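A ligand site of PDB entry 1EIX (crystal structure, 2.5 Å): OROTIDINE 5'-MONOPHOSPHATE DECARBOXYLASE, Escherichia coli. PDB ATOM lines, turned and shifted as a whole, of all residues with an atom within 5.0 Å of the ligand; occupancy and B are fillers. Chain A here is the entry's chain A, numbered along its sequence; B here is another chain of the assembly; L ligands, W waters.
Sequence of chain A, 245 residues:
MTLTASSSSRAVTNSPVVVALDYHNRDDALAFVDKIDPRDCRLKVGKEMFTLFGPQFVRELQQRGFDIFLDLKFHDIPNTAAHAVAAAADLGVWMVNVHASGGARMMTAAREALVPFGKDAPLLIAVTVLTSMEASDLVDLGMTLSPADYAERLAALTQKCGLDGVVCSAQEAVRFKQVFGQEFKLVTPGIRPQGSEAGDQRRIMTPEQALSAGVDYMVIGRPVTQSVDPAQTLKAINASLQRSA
The side-chain carboxylate (OD2) of Asp 71 lies close to an oxygen (O10) of the ligand (3.3 Å).
Ala 20 touches the ligand (CB to C2, 3.5 Å).
Leu 130 touches the ligand (CA to O9, 3.3 Å).
Val 167 touches the ligand (CG1 to C8, 3.8 Å).
CB of Pro 189 touches C6 of the ligand (3.5 Å).
CG1 of Val 219 touches O5 of the ligand (3.5 Å).
C of Ile 220 touches O2 of the ligand (3.9 Å).
CD1 of Ile 77 of chain B touches O8 of the ligand, 3.3 Å away.
18 residues have an atom within 4 Å of the ligand: Ala 20, Asp 22, Lys 44, Asp 71, Lys 73, Leu 130, Thr 131, Val 167, Pro 189, Arg 192, Gln 201, Val 219, Ile 220, Gly 221, Arg 222, Asp 76 of chain B, Ile 77 of chain B and Thr 80 of chain B.
Along chain A the residues within 4 Å of the ligand span positions 20 to 222.
Water W1 bridges an oxygen (O3) of the ligand and the side-chain carboxylate (OD2) of Asp 22.
Water W2 lies within hydrogen-bond range of the backbone carbonyl oxygen of Val 219 (2.5 Å), an oxygen (O2) of the ligand (2.6 Å), the backbone NH of Gly 190 (2.8 Å) and the backbone NH of Ile 191 (3.0 Å).
Water W4 lies within hydrogen-bond range of an oxygen (O6) of the ligand (2.6 Å), the side-chain amino group (NZ) of Lys 44 (3.0 Å) and the side-chain carboxylate (OD2) of Asp 71 (3.5 Å).
Water W3 lies within hydrogen-bond range of the side-chain amide nitrogen (ND2) of Asn 97 (2.5 Å), an oxygen (O10) of the ligand (3.0 Å) and the side-chain carboxylate (OD1) of Asp 71 (3.1 Å).
O2 of the ligand is in salt-bridge range of NH2 of Arg 192 (2.4 Å).
NZ of Lys 44 is in hydrogen-bond range of O6 of the ligand, at 2.6 Å.
OG1 of Thr 80 of chain B sits at hydrogen-bond distance from O7 of the ligand (2.6 Å).
The backbone NH (N) of Arg 222 lies within hydrogen-bond range of an oxygen (O3) of the ligand, 2.8 Å away.
NH2 of Arg 222 lies within salt-bridge range of O1 of the ligand.
The side-chain amino group of Lys 73 is in hydrogen-bond range of an oxygen (O10) of the ligand, 2.7 Å away.
An oxygen (O7) of the ligand is in hydrogen-bond range of the side-chain carboxylate (OD1) of Asp 76 of chain B, at 2.8 Å.
N of Thr 131 sits at hydrogen-bond distance from O9 of the ligand (3.0 Å).
OG1 of Thr 131 lies within hydrogen-bond range of N2 of the ligand, at 2.9 Å.
O8 of the ligand sits at hydrogen-bond distance from NE2 of Gln 201, at 2.9 Å.
An oxygen (O2) of the ligand sits at hydrogen-bond distance from the backbone NH of Gly 221 (2.9 Å).
O6 of the ligand lies within hydrogen-bond range of OD2 of Asp 22, at 2.9 Å.
NZ of Lys 44 lies within salt-bridge range of OD2 of Asp 71, 2.8 Å away.
The side-chain carboxylate (OD2) of Asp 76 of chain B lies within salt-bridge range of the side-chain amino group (NZ) of Lys 73 (2.9 Å).
The side-chain amino group (NZ) of Lys 73 lies within salt-bridge range of the side-chain carboxylate (OD1) of Asp 71, at 2.5 Å.
OG1 of Thr 131 lies within hydrogen-bond range of OE1 of Gln 201.
The backbone NH of Ala 20 is in hydrogen-bond range of the backbone carbonyl oxygen of Ile 220 (2.9 Å).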
ATOM      1  N   ALA A  20      15.736  19.545  21.555  1.00  0.00           N
ATOM      2  CA  ALA A  20      16.273  20.018  20.295  1.00  0.00           C
ATOM      3  C   ALA A  20      17.783  19.829  20.246  1.00  0.00           C
ATOM      4  O   ALA A  20      18.495  20.573  20.924  1.00  0.00           O
ATOM      5  CB  ALA A  20      15.936  21.474  20.111  1.00  0.00           C
ATOM      6  N   ASP A  22      20.657  20.827  18.864  1.00  0.00           N
ATOM      7  CA  ASP A  22      21.184  21.908  18.023  1.00  0.00           C
ATOM      8  C   ASP A  22      22.658  22.185  18.287  1.00  0.00           C
ATOM      9  O   ASP A  22      23.026  23.284  18.687  1.00  0.00           O
ATOM     10  CB  ASP A  22      20.396  23.216  18.235  1.00  0.00           C
ATOM     11  CG  ASP A  22      18.946  23.115  17.756  1.00  0.00           C
ATOM     12  OD1 ASP A  22      18.573  22.092  17.139  1.00  0.00           O
ATOM     13  OD2 ASP A  22      18.191  24.074  17.990  1.00  0.00           O
ATOM     14  N   LYS A  44      15.116  15.767  18.577  1.00  0.00           N
ATOM     15  CA  LYS A  44      14.761  16.571  17.415  1.00  0.00           C
ATOM     16  C   LYS A  44      16.018  16.959  16.658  1.00  0.00           C
ATOM     17  O   LYS A  44      16.916  17.600  17.207  1.00  0.00           O
ATOM     18  CB  LYS A  44      13.986  17.801  17.874  1.00  0.00           C
ATOM     19  CG  LYS A  44      13.549  18.734  16.782  1.00  0.00           C
ATOM     20  CD  LYS A  44      12.893  19.955  17.433  1.00  0.00           C
ATOM     21  CE  LYS A  44      13.060  21.187  16.585  1.00  0.00           C
ATOM     22  NZ  LYS A  44      14.494  21.366  16.186  1.00  0.00           N
ATOM     23  N   ASP A  71      13.157  17.839  11.923  1.00  0.00           N
ATOM     24  CA  ASP A  71      12.645  19.193  11.844  1.00  0.00           C
ATOM     25  C   ASP A  71      13.274  20.009  10.733  1.00  0.00           C
ATOM     26  O   ASP A  71      14.208  20.765  10.966  1.00  0.00           O
ATOM     27  CB  ASP A  71      12.858  19.871  13.210  1.00  0.00           C
ATOM     28  CG  ASP A  71      12.434  21.312  13.215  1.00  0.00           C
ATOM     29  OD1 ASP A  71      11.456  21.635  12.513  1.00  0.00           O
ATOM     30  OD2 ASP A  71      13.048  22.122  13.935  1.00  0.00           O
ATOM     31  N   LYS A  73      11.123  21.661   8.450  1.00  0.00           N
ATOM     32  CA  LYS A  73      10.082  22.592   8.047  1.00  0.00           C
ATOM     33  C   LYS A  73       9.994  22.771   6.532  1.00  0.00           C
ATOM     34  O   LYS A  73      10.147  23.870   6.024  1.00  0.00           O
ATOM     35  CB  LYS A  73      10.339  23.947   8.709  1.00  0.00           C
ATOM     36  CG  LYS A  73      10.456  23.856  10.227  1.00  0.00           C
ATOM     37  CD  LYS A  73      10.721  25.200  10.870  1.00  0.00           C
ATOM     38  CE  LYS A  73      10.611  25.111  12.394  1.00  0.00           C
ATOM     39  NZ  LYS A  73      11.544  24.129  12.993  1.00  0.00           N
ATOM     40  N   ASN A  97       8.406  17.468   9.776  1.00  0.00           N
ATOM     41  CA  ASN A  97       7.900  18.832   9.635  1.00  0.00           C
ATOM     42  C   ASN A  97       7.485  19.299   8.240  1.00  0.00           C
ATOM     43  O   ASN A  97       7.778  18.656   7.240  1.00  0.00           O
ATOM     44  CB  ASN A  97       8.963  19.804  10.150  1.00  0.00           C
ATOM     45  CG  ASN A  97       8.450  20.671  11.268  1.00  0.00           C
ATOM     46  OD1 ASN A  97       7.328  21.160  11.201  1.00  0.00           O
ATOM     47  ND2 ASN A  97       9.264  20.860  12.298  1.00  0.00           N
ATOM     48  N   VAL A 127       4.116  23.682  10.743  1.00  0.00           N
ATOM     49  CA  VAL A 127       4.531  24.816  11.542  1.00  0.00           C
ATOM     50  C   VAL A 127       3.550  25.921  11.227  1.00  0.00           C
ATOM     51  O   VAL A 127       3.210  26.144  10.068  1.00  0.00           O
ATOM     52  CB  VAL A 127       5.925  25.296  11.141  1.00  0.00           C
ATOM     53  CG1 VAL A 127       6.270  26.559  11.929  1.00  0.00           C
ATOM     54  CG2 VAL A 127       6.961  24.210  11.400  1.00  0.00           C
ATOM     55  N   VAL A 129       3.004  29.658  13.188  1.00  0.00           N
ATOM     56  CA  VAL A 129       3.777  30.880  13.331  1.00  0.00           C
ATOM     57  C   VAL A 129       4.931  30.603  14.294  1.00  0.00           C
ATOM     58  O   VAL A 129       4.723  30.153  15.408  1.00  0.00           O
ATOM     59  CB  VAL A 129       2.904  32.026  13.880  1.00  0.00           C
ATOM     60  CG1 VAL A 129       3.750  33.286  14.074  1.00  0.00           C
ATOM     61  CG2 VAL A 129       1.757  32.308  12.905  1.00  0.00           C
ATOM     62  N   LEU A 130       6.153  30.860  13.847  1.00  0.00           N
ATOM     63  CA  LEU A 130       7.326  30.610  14.682  1.00  0.00           C
ATOM     64  C   LEU A 130       7.234  31.377  16.010  1.00  0.00           C
ATOM     65  O   LEU A 130       6.851  32.551  16.052  1.00  0.00           O
ATOM     66  CB  LEU A 130       8.597  31.014  13.932  1.00  0.00           C
ATOM     67  CG  LEU A 130       8.866  30.206  12.658  1.00  0.00           C
ATOM     68  CD1 LEU A 130      10.041  30.824  11.902  1.00  0.00           C
ATOM     69  CD2 LEU A 130       9.144  28.746  13.017  1.00  0.00           C
ATOM     70  N   THR A 131       7.581  30.694  17.090  1.00  0.00           N
ATOM     71  CA  THR A 131       7.524  31.255  18.433  1.00  0.00           C
ATOM     72  C   THR A 131       8.447  32.441  18.660  1.00  0.00           C
ATOM     73  O   THR A 131       8.439  33.065  19.726  1.00  0.00           O
ATOM     74  CB  THR A 131       7.851  30.191  19.471  1.00  0.00           C
ATOM     75  OG1 THR A 131       9.147  29.666  19.194  1.00  0.00           O
ATOM     76  CG2 THR A 131       6.827  29.074  19.428  1.00  0.00           C
ATOM     77  N   VAL A 167       2.753  22.931  14.843  1.00  0.00           N
ATOM     78  CA  VAL A 167       3.813  23.412  15.701  1.00  0.00           C
ATOM     79  C   VAL A 167       3.347  24.837  15.975  1.00  0.00           C
ATOM     80  O   VAL A 167       2.905  25.521  15.060  1.00  0.00           O
ATOM     81  CB  VAL A 167       5.189  23.471  15.001  1.00  0.00           C
ATOM     82  CG1 VAL A 167       6.196  24.162  15.904  1.00  0.00           C
ATOM     83  CG2 VAL A 167       5.676  22.062  14.694  1.00  0.00           C
ATOM     84  N   PRO A 189       7.412  24.774  20.975  1.00  0.00           N
ATOM     85  CA  PRO A 189       8.777  25.171  21.342  1.00  0.00           C
ATOM     86  C   PRO A 189       8.585  26.479  22.127  1.00  0.00           C
ATOM     87  O   PRO A 189       7.474  26.783  22.540  1.00  0.00           O
ATOM     88  CB  PRO A 189       9.451  25.411  19.988  1.00  0.00           C
ATOM     89  CG  PRO A 189       8.582  24.663  19.009  1.00  0.00           C
ATOM     90  CD  PRO A 189       7.205  24.943  19.526  1.00  0.00           C
ATOM     91  N   GLY A 190       9.644  27.251  22.292  1.00  0.00           N
ATOM     92  CA  GLY A 190       9.507  28.483  23.059  1.00  0.00           C
ATOM     93  C   GLY A 190       9.273  28.146  24.519  1.00  0.00           C
ATOM     94  O   GLY A 190       8.492  28.806  25.204  1.00  0.00           O
ATOM     95  N   ILE A 191       9.940  27.106  24.984  1.00  0.00           N
ATOM     96  CA  ILE A 191       9.831  26.667  26.368  1.00  0.00           C
ATOM     97  C   ILE A 191      11.017  27.168  27.179  1.00  0.00           C
ATOM     98  O   ILE A 191      12.181  26.850  26.888  1.00  0.00           O
ATOM     99  CB  ILE A 191       9.817  25.141  26.432  1.00  0.00           C
ATOM    100  CG1 ILE A 191       8.760  24.590  25.464  1.00  0.00           C
ATOM    101  CG2 ILE A 191       9.617  24.692  27.871  1.00  0.00           C
ATOM    102  CD1 ILE A 191       7.384  25.190  25.638  1.00  0.00           C
ATOM    103  N   ARG A 192      10.727  27.973  28.200  1.00  0.00           N
ATOM    104  CA  ARG A 192      11.774  28.523  29.047  1.00  0.00           C
ATOM    105  C   ARG A 192      11.443  28.319  30.527  1.00  0.00           C
ATOM    106  O   ARG A 192      10.494  28.915  31.045  1.00  0.00           O
ATOM    107  CB  ARG A 192      11.946  30.028  28.830  1.00  0.00           C
ATOM    108  CG  ARG A 192      12.097  30.528  27.393  1.00  0.00           C
ATOM    109  CD  ARG A 192      13.526  30.454  26.867  1.00  0.00           C
ATOM    110  NE  ARG A 192      13.758  29.157  26.262  1.00  0.00           N
ATOM    111  CZ  ARG A 192      14.513  28.951  25.190  1.00  0.00           C
ATOM    112  NH1 ARG A 192      15.129  29.959  24.583  1.00  0.00           N
ATOM    113  NH2 ARG A 192      14.637  27.724  24.728  1.00  0.00           N
ATOM    114  N   GLN A 201      13.692  33.751  21.201  1.00  0.00           N
ATOM    115  CA  GLN A 201      12.350  33.247  21.473  1.00  0.00           C
ATOM    116  C   GLN A 201      11.440  34.386  21.943  1.00  0.00           C
ATOM    117  O   GLN A 201      11.879  35.254  22.698  1.00  0.00           O
ATOM    118  CB  GLN A 201      12.423  32.159  22.533  1.00  0.00           C
ATOM    119  CG  GLN A 201      11.486  30.991  22.324  1.00  0.00           C
ATOM    120  CD  GLN A 201      11.592  30.414  20.931  1.00  0.00           C
ATOM    121  OE1 GLN A 201      11.084  30.982  19.968  1.00  0.00           O
ATOM    122  NE2 GLN A 201      12.270  29.266  20.805  1.00  0.00           N
ATOM    123  N   VAL A 219       9.036  21.412  22.972  1.00  0.00           N
ATOM    124  CA  VAL A 219      10.387  21.348  22.457  1.00  0.00           C
ATOM    125  C   VAL A 219      11.296  22.241  23.286  1.00  0.00           C
ATOM    126  O   VAL A 219      11.042  23.443  23.411  1.00  0.00           O
ATOM    127  CB  VAL A 219      10.438  21.798  20.981  1.00  0.00           C
ATOM    128  CG1 VAL A 219      11.882  21.814  20.480  1.00  0.00           C
ATOM    129  CG2 VAL A 219       9.585  20.859  20.139  1.00  0.00           C
ATOM    130  N   ILE A 220      12.337  21.646  23.842  1.00  0.00           N
ATOM    131  CA  ILE A 220      13.293  22.386  24.657  1.00  0.00           C
ATOM    132  C   ILE A 220      14.728  22.205  24.141  1.00  0.00           C
ATOM    133  O   ILE A 220      15.199  21.080  23.935  1.00  0.00           O
ATOM    134  CB  ILE A 220      13.236  21.928  26.135  1.00  0.00           C
ATOM    135  CG1 ILE A 220      11.792  21.999  26.641  1.00  0.00           C
ATOM    136  CG2 ILE A 220      14.137  22.816  26.975  1.00  0.00           C
ATOM    137  CD1 ILE A 220      11.612  21.421  28.042  1.00  0.00           C
ATOM    138  N   GLY A 221      15.413  23.329  23.938  1.00  0.00           N
ATOM    139  CA  GLY A 221      16.765  23.285  23.460  1.00  0.00           C
ATOM    140  C   GLY A 221      17.800  23.842  24.418  1.00  0.00           C
ATOM    141  O   GLY A 221      18.256  23.142  25.325  1.00  0.00           O
ATOM    142  N   ARG A 222      18.155  25.106  24.229  1.00  0.00           N
ATOM    143  CA  ARG A 222      19.159  25.753  25.049  1.00  0.00           C
ATOM    144  C   ARG A 222      19.071  25.597  26.564  1.00  0.00           C
ATOM    145  O   ARG A 222      20.091  25.411  27.230  1.00  0.00           O
ATOM    146  CB  ARG A 222      19.235  27.237  24.676  1.00  0.00           C
ATOM    147  CG  ARG A 222      19.995  27.443  23.377  1.00  0.00           C
ATOM    148  CD  ARG A 222      19.730  28.786  22.734  1.00  0.00           C
ATOM    149  NE  ARG A 222      18.413  28.854  22.118  1.00  0.00           N
ATOM    150  CZ  ARG A 222      18.027  29.838  21.310  1.00  0.00           C
ATOM    151  NH1 ARG A 222      18.857  30.826  21.036  1.00  0.00           N
ATOM    152  NH2 ARG A 222      16.803  29.828  20.788  1.00  0.00           N
ATOM    153  N   PRO A 223      17.856  25.652  27.148  1.00  0.00           N
ATOM    154  CA  PRO A 223      17.773  25.495  28.612  1.00  0.00           C
ATOM    155  C   PRO A 223      18.430  24.188  29.075  1.00  0.00           C
ATOM    156  O   PRO A 223      18.925  24.087  30.197  1.00  0.00           O
ATOM    157  CB  PRO A 223      16.273  25.514  28.875  1.00  0.00           C
ATOM    158  CG  PRO A 223      15.767  26.468  27.822  1.00  0.00           C
ATOM    159  CD  PRO A 223      16.550  26.039  26.586  1.00  0.00           C
ATOM    160  N   ASP B  76      13.192  29.429   9.890  1.00  0.00           N
ATOM    161  CA  ASP B  76      13.091  29.059  11.292  1.00  0.00           C
ATOM    162  C   ASP B  76      13.360  30.260  12.175  1.00  0.00           C
ATOM    163  O   ASP B  76      13.409  31.404  11.712  1.00  0.00           O
ATOM    164  CB  ASP B  76      14.134  27.968  11.572  1.00  0.00           C
ATOM    165  CG  ASP B  76      13.624  26.869  12.468  1.00  0.00           C
ATOM    166  OD1 ASP B  76      13.039  27.186  13.525  1.00  0.00           O
ATOM    167  OD2 ASP B  76      13.808  25.678  12.129  1.00  0.00           O
ATOM    168  N   ILE B  77      13.533  30.005  13.467  1.00  0.00           N
ATOM    169  CA  ILE B  77      13.823  31.077  14.393  1.00  0.00           C
ATOM    170  C   ILE B  77      15.236  31.576  14.099  1.00  0.00           C
ATOM    171  O   ILE B  77      16.108  30.817  13.663  1.00  0.00           O
ATOM    172  CB  ILE B  77      13.751  30.602  15.854  1.00  0.00           C
ATOM    173  CG1 ILE B  77      14.786  29.498  16.096  1.00  0.00           C
ATOM    174  CG2 ILE B  77      12.361  30.111  16.155  1.00  0.00           C
ATOM    175  CD1 ILE B  77      15.013  29.194  17.558  1.00  0.00           C
ATOM    176  N   THR B  80      18.265  29.328  14.747  1.00  0.00           N
ATOM    177  CA  THR B  80      18.393  28.146  13.900  1.00  0.00           C
ATOM    178  C   THR B  80      18.805  28.511  12.480  1.00  0.00           C
ATOM    179  O   THR B  80      19.595  27.812  11.863  1.00  0.00           O
ATOM    180  CB  THR B  80      17.075  27.361  13.856  1.00  0.00           C
ATOM    181  OG1 THR B  80      16.807  26.808  15.154  1.00  0.00           O
ATOM    182  CG2 THR B  80      17.164  26.227  12.839  1.00  0.00           C
HETATM  183  P1  LIG L   1      15.297  26.676  22.022  1.00  0.00           P
HETATM  184  O1  LIG L   1      15.079  28.205  22.005  1.00  0.00           O
HETATM  185  O2  LIG L   1      14.511  25.949  23.061  1.00  0.00           O
HETATM  186  O3  LIG L   1      16.763  26.392  22.205  1.00  0.00           O
HETATM  187  O4  LIG L   1      14.822  26.235  20.570  1.00  0.00           O
HETATM  188  C1  LIG L   1      14.871  24.846  20.282  1.00  0.00           C
HETATM  189  C2  LIG L   1      14.471  24.438  18.934  1.00  0.00           C
HETATM  190  O5  LIG L   1      12.959  24.619  18.659  1.00  0.00           O
HETATM  191  C3  LIG L   1      15.199  24.879  17.705  1.00  0.00           C
HETATM  192  O6  LIG L   1      15.471  23.694  16.926  1.00  0.00           O
HETATM  193  C4  LIG L   1      14.162  25.730  16.939  1.00  0.00           C
HETATM  194  O7  LIG L   1      14.348  25.922  15.588  1.00  0.00           O
HETATM  195  C5  LIG L   1      12.876  25.022  17.277  1.00  0.00           C
HETATM  196  N1  LIG L   1      11.583  25.819  16.996  1.00  0.00           N
HETATM  197  C6  LIG L   1      11.386  27.057  17.631  1.00  0.00           C
HETATM  198  O8  LIG L   1      12.276  27.593  18.475  1.00  0.00           O
HETATM  199  N2  LIG L   1      10.204  27.751  17.346  1.00  0.00           N
HETATM  200  C7  LIG L   1       9.263  27.233  16.480  1.00  0.00           C
HETATM  201  O9  LIG L   1       8.238  27.881  16.260  1.00  0.00           O
HETATM  202  C8  LIG L   1       9.517  25.955  15.861  1.00  0.00           C
HETATM  203  C9  LIG L   1      10.700  25.324  16.186  1.00  0.00           C
HETATM  204  O10 LIG L   1      10.941  24.123  15.594  1.00  0.00           O
HETATM  205  O   HOH W   1      18.252  25.075  20.694  1.00  0.00           O
HETATM  206  O   HOH W   2      11.913  25.813  23.068  1.00  0.00           O
HETATM  207  O   HOH W   3       9.237  21.821  14.657  1.00  0.00           O
HETATM  208  O   HOH W   4      16.321  23.056  14.547  1.00  0.00           O
HETATM  209  O   HOH W   5       5.246  27.450  15.619  1.00  0.00           O
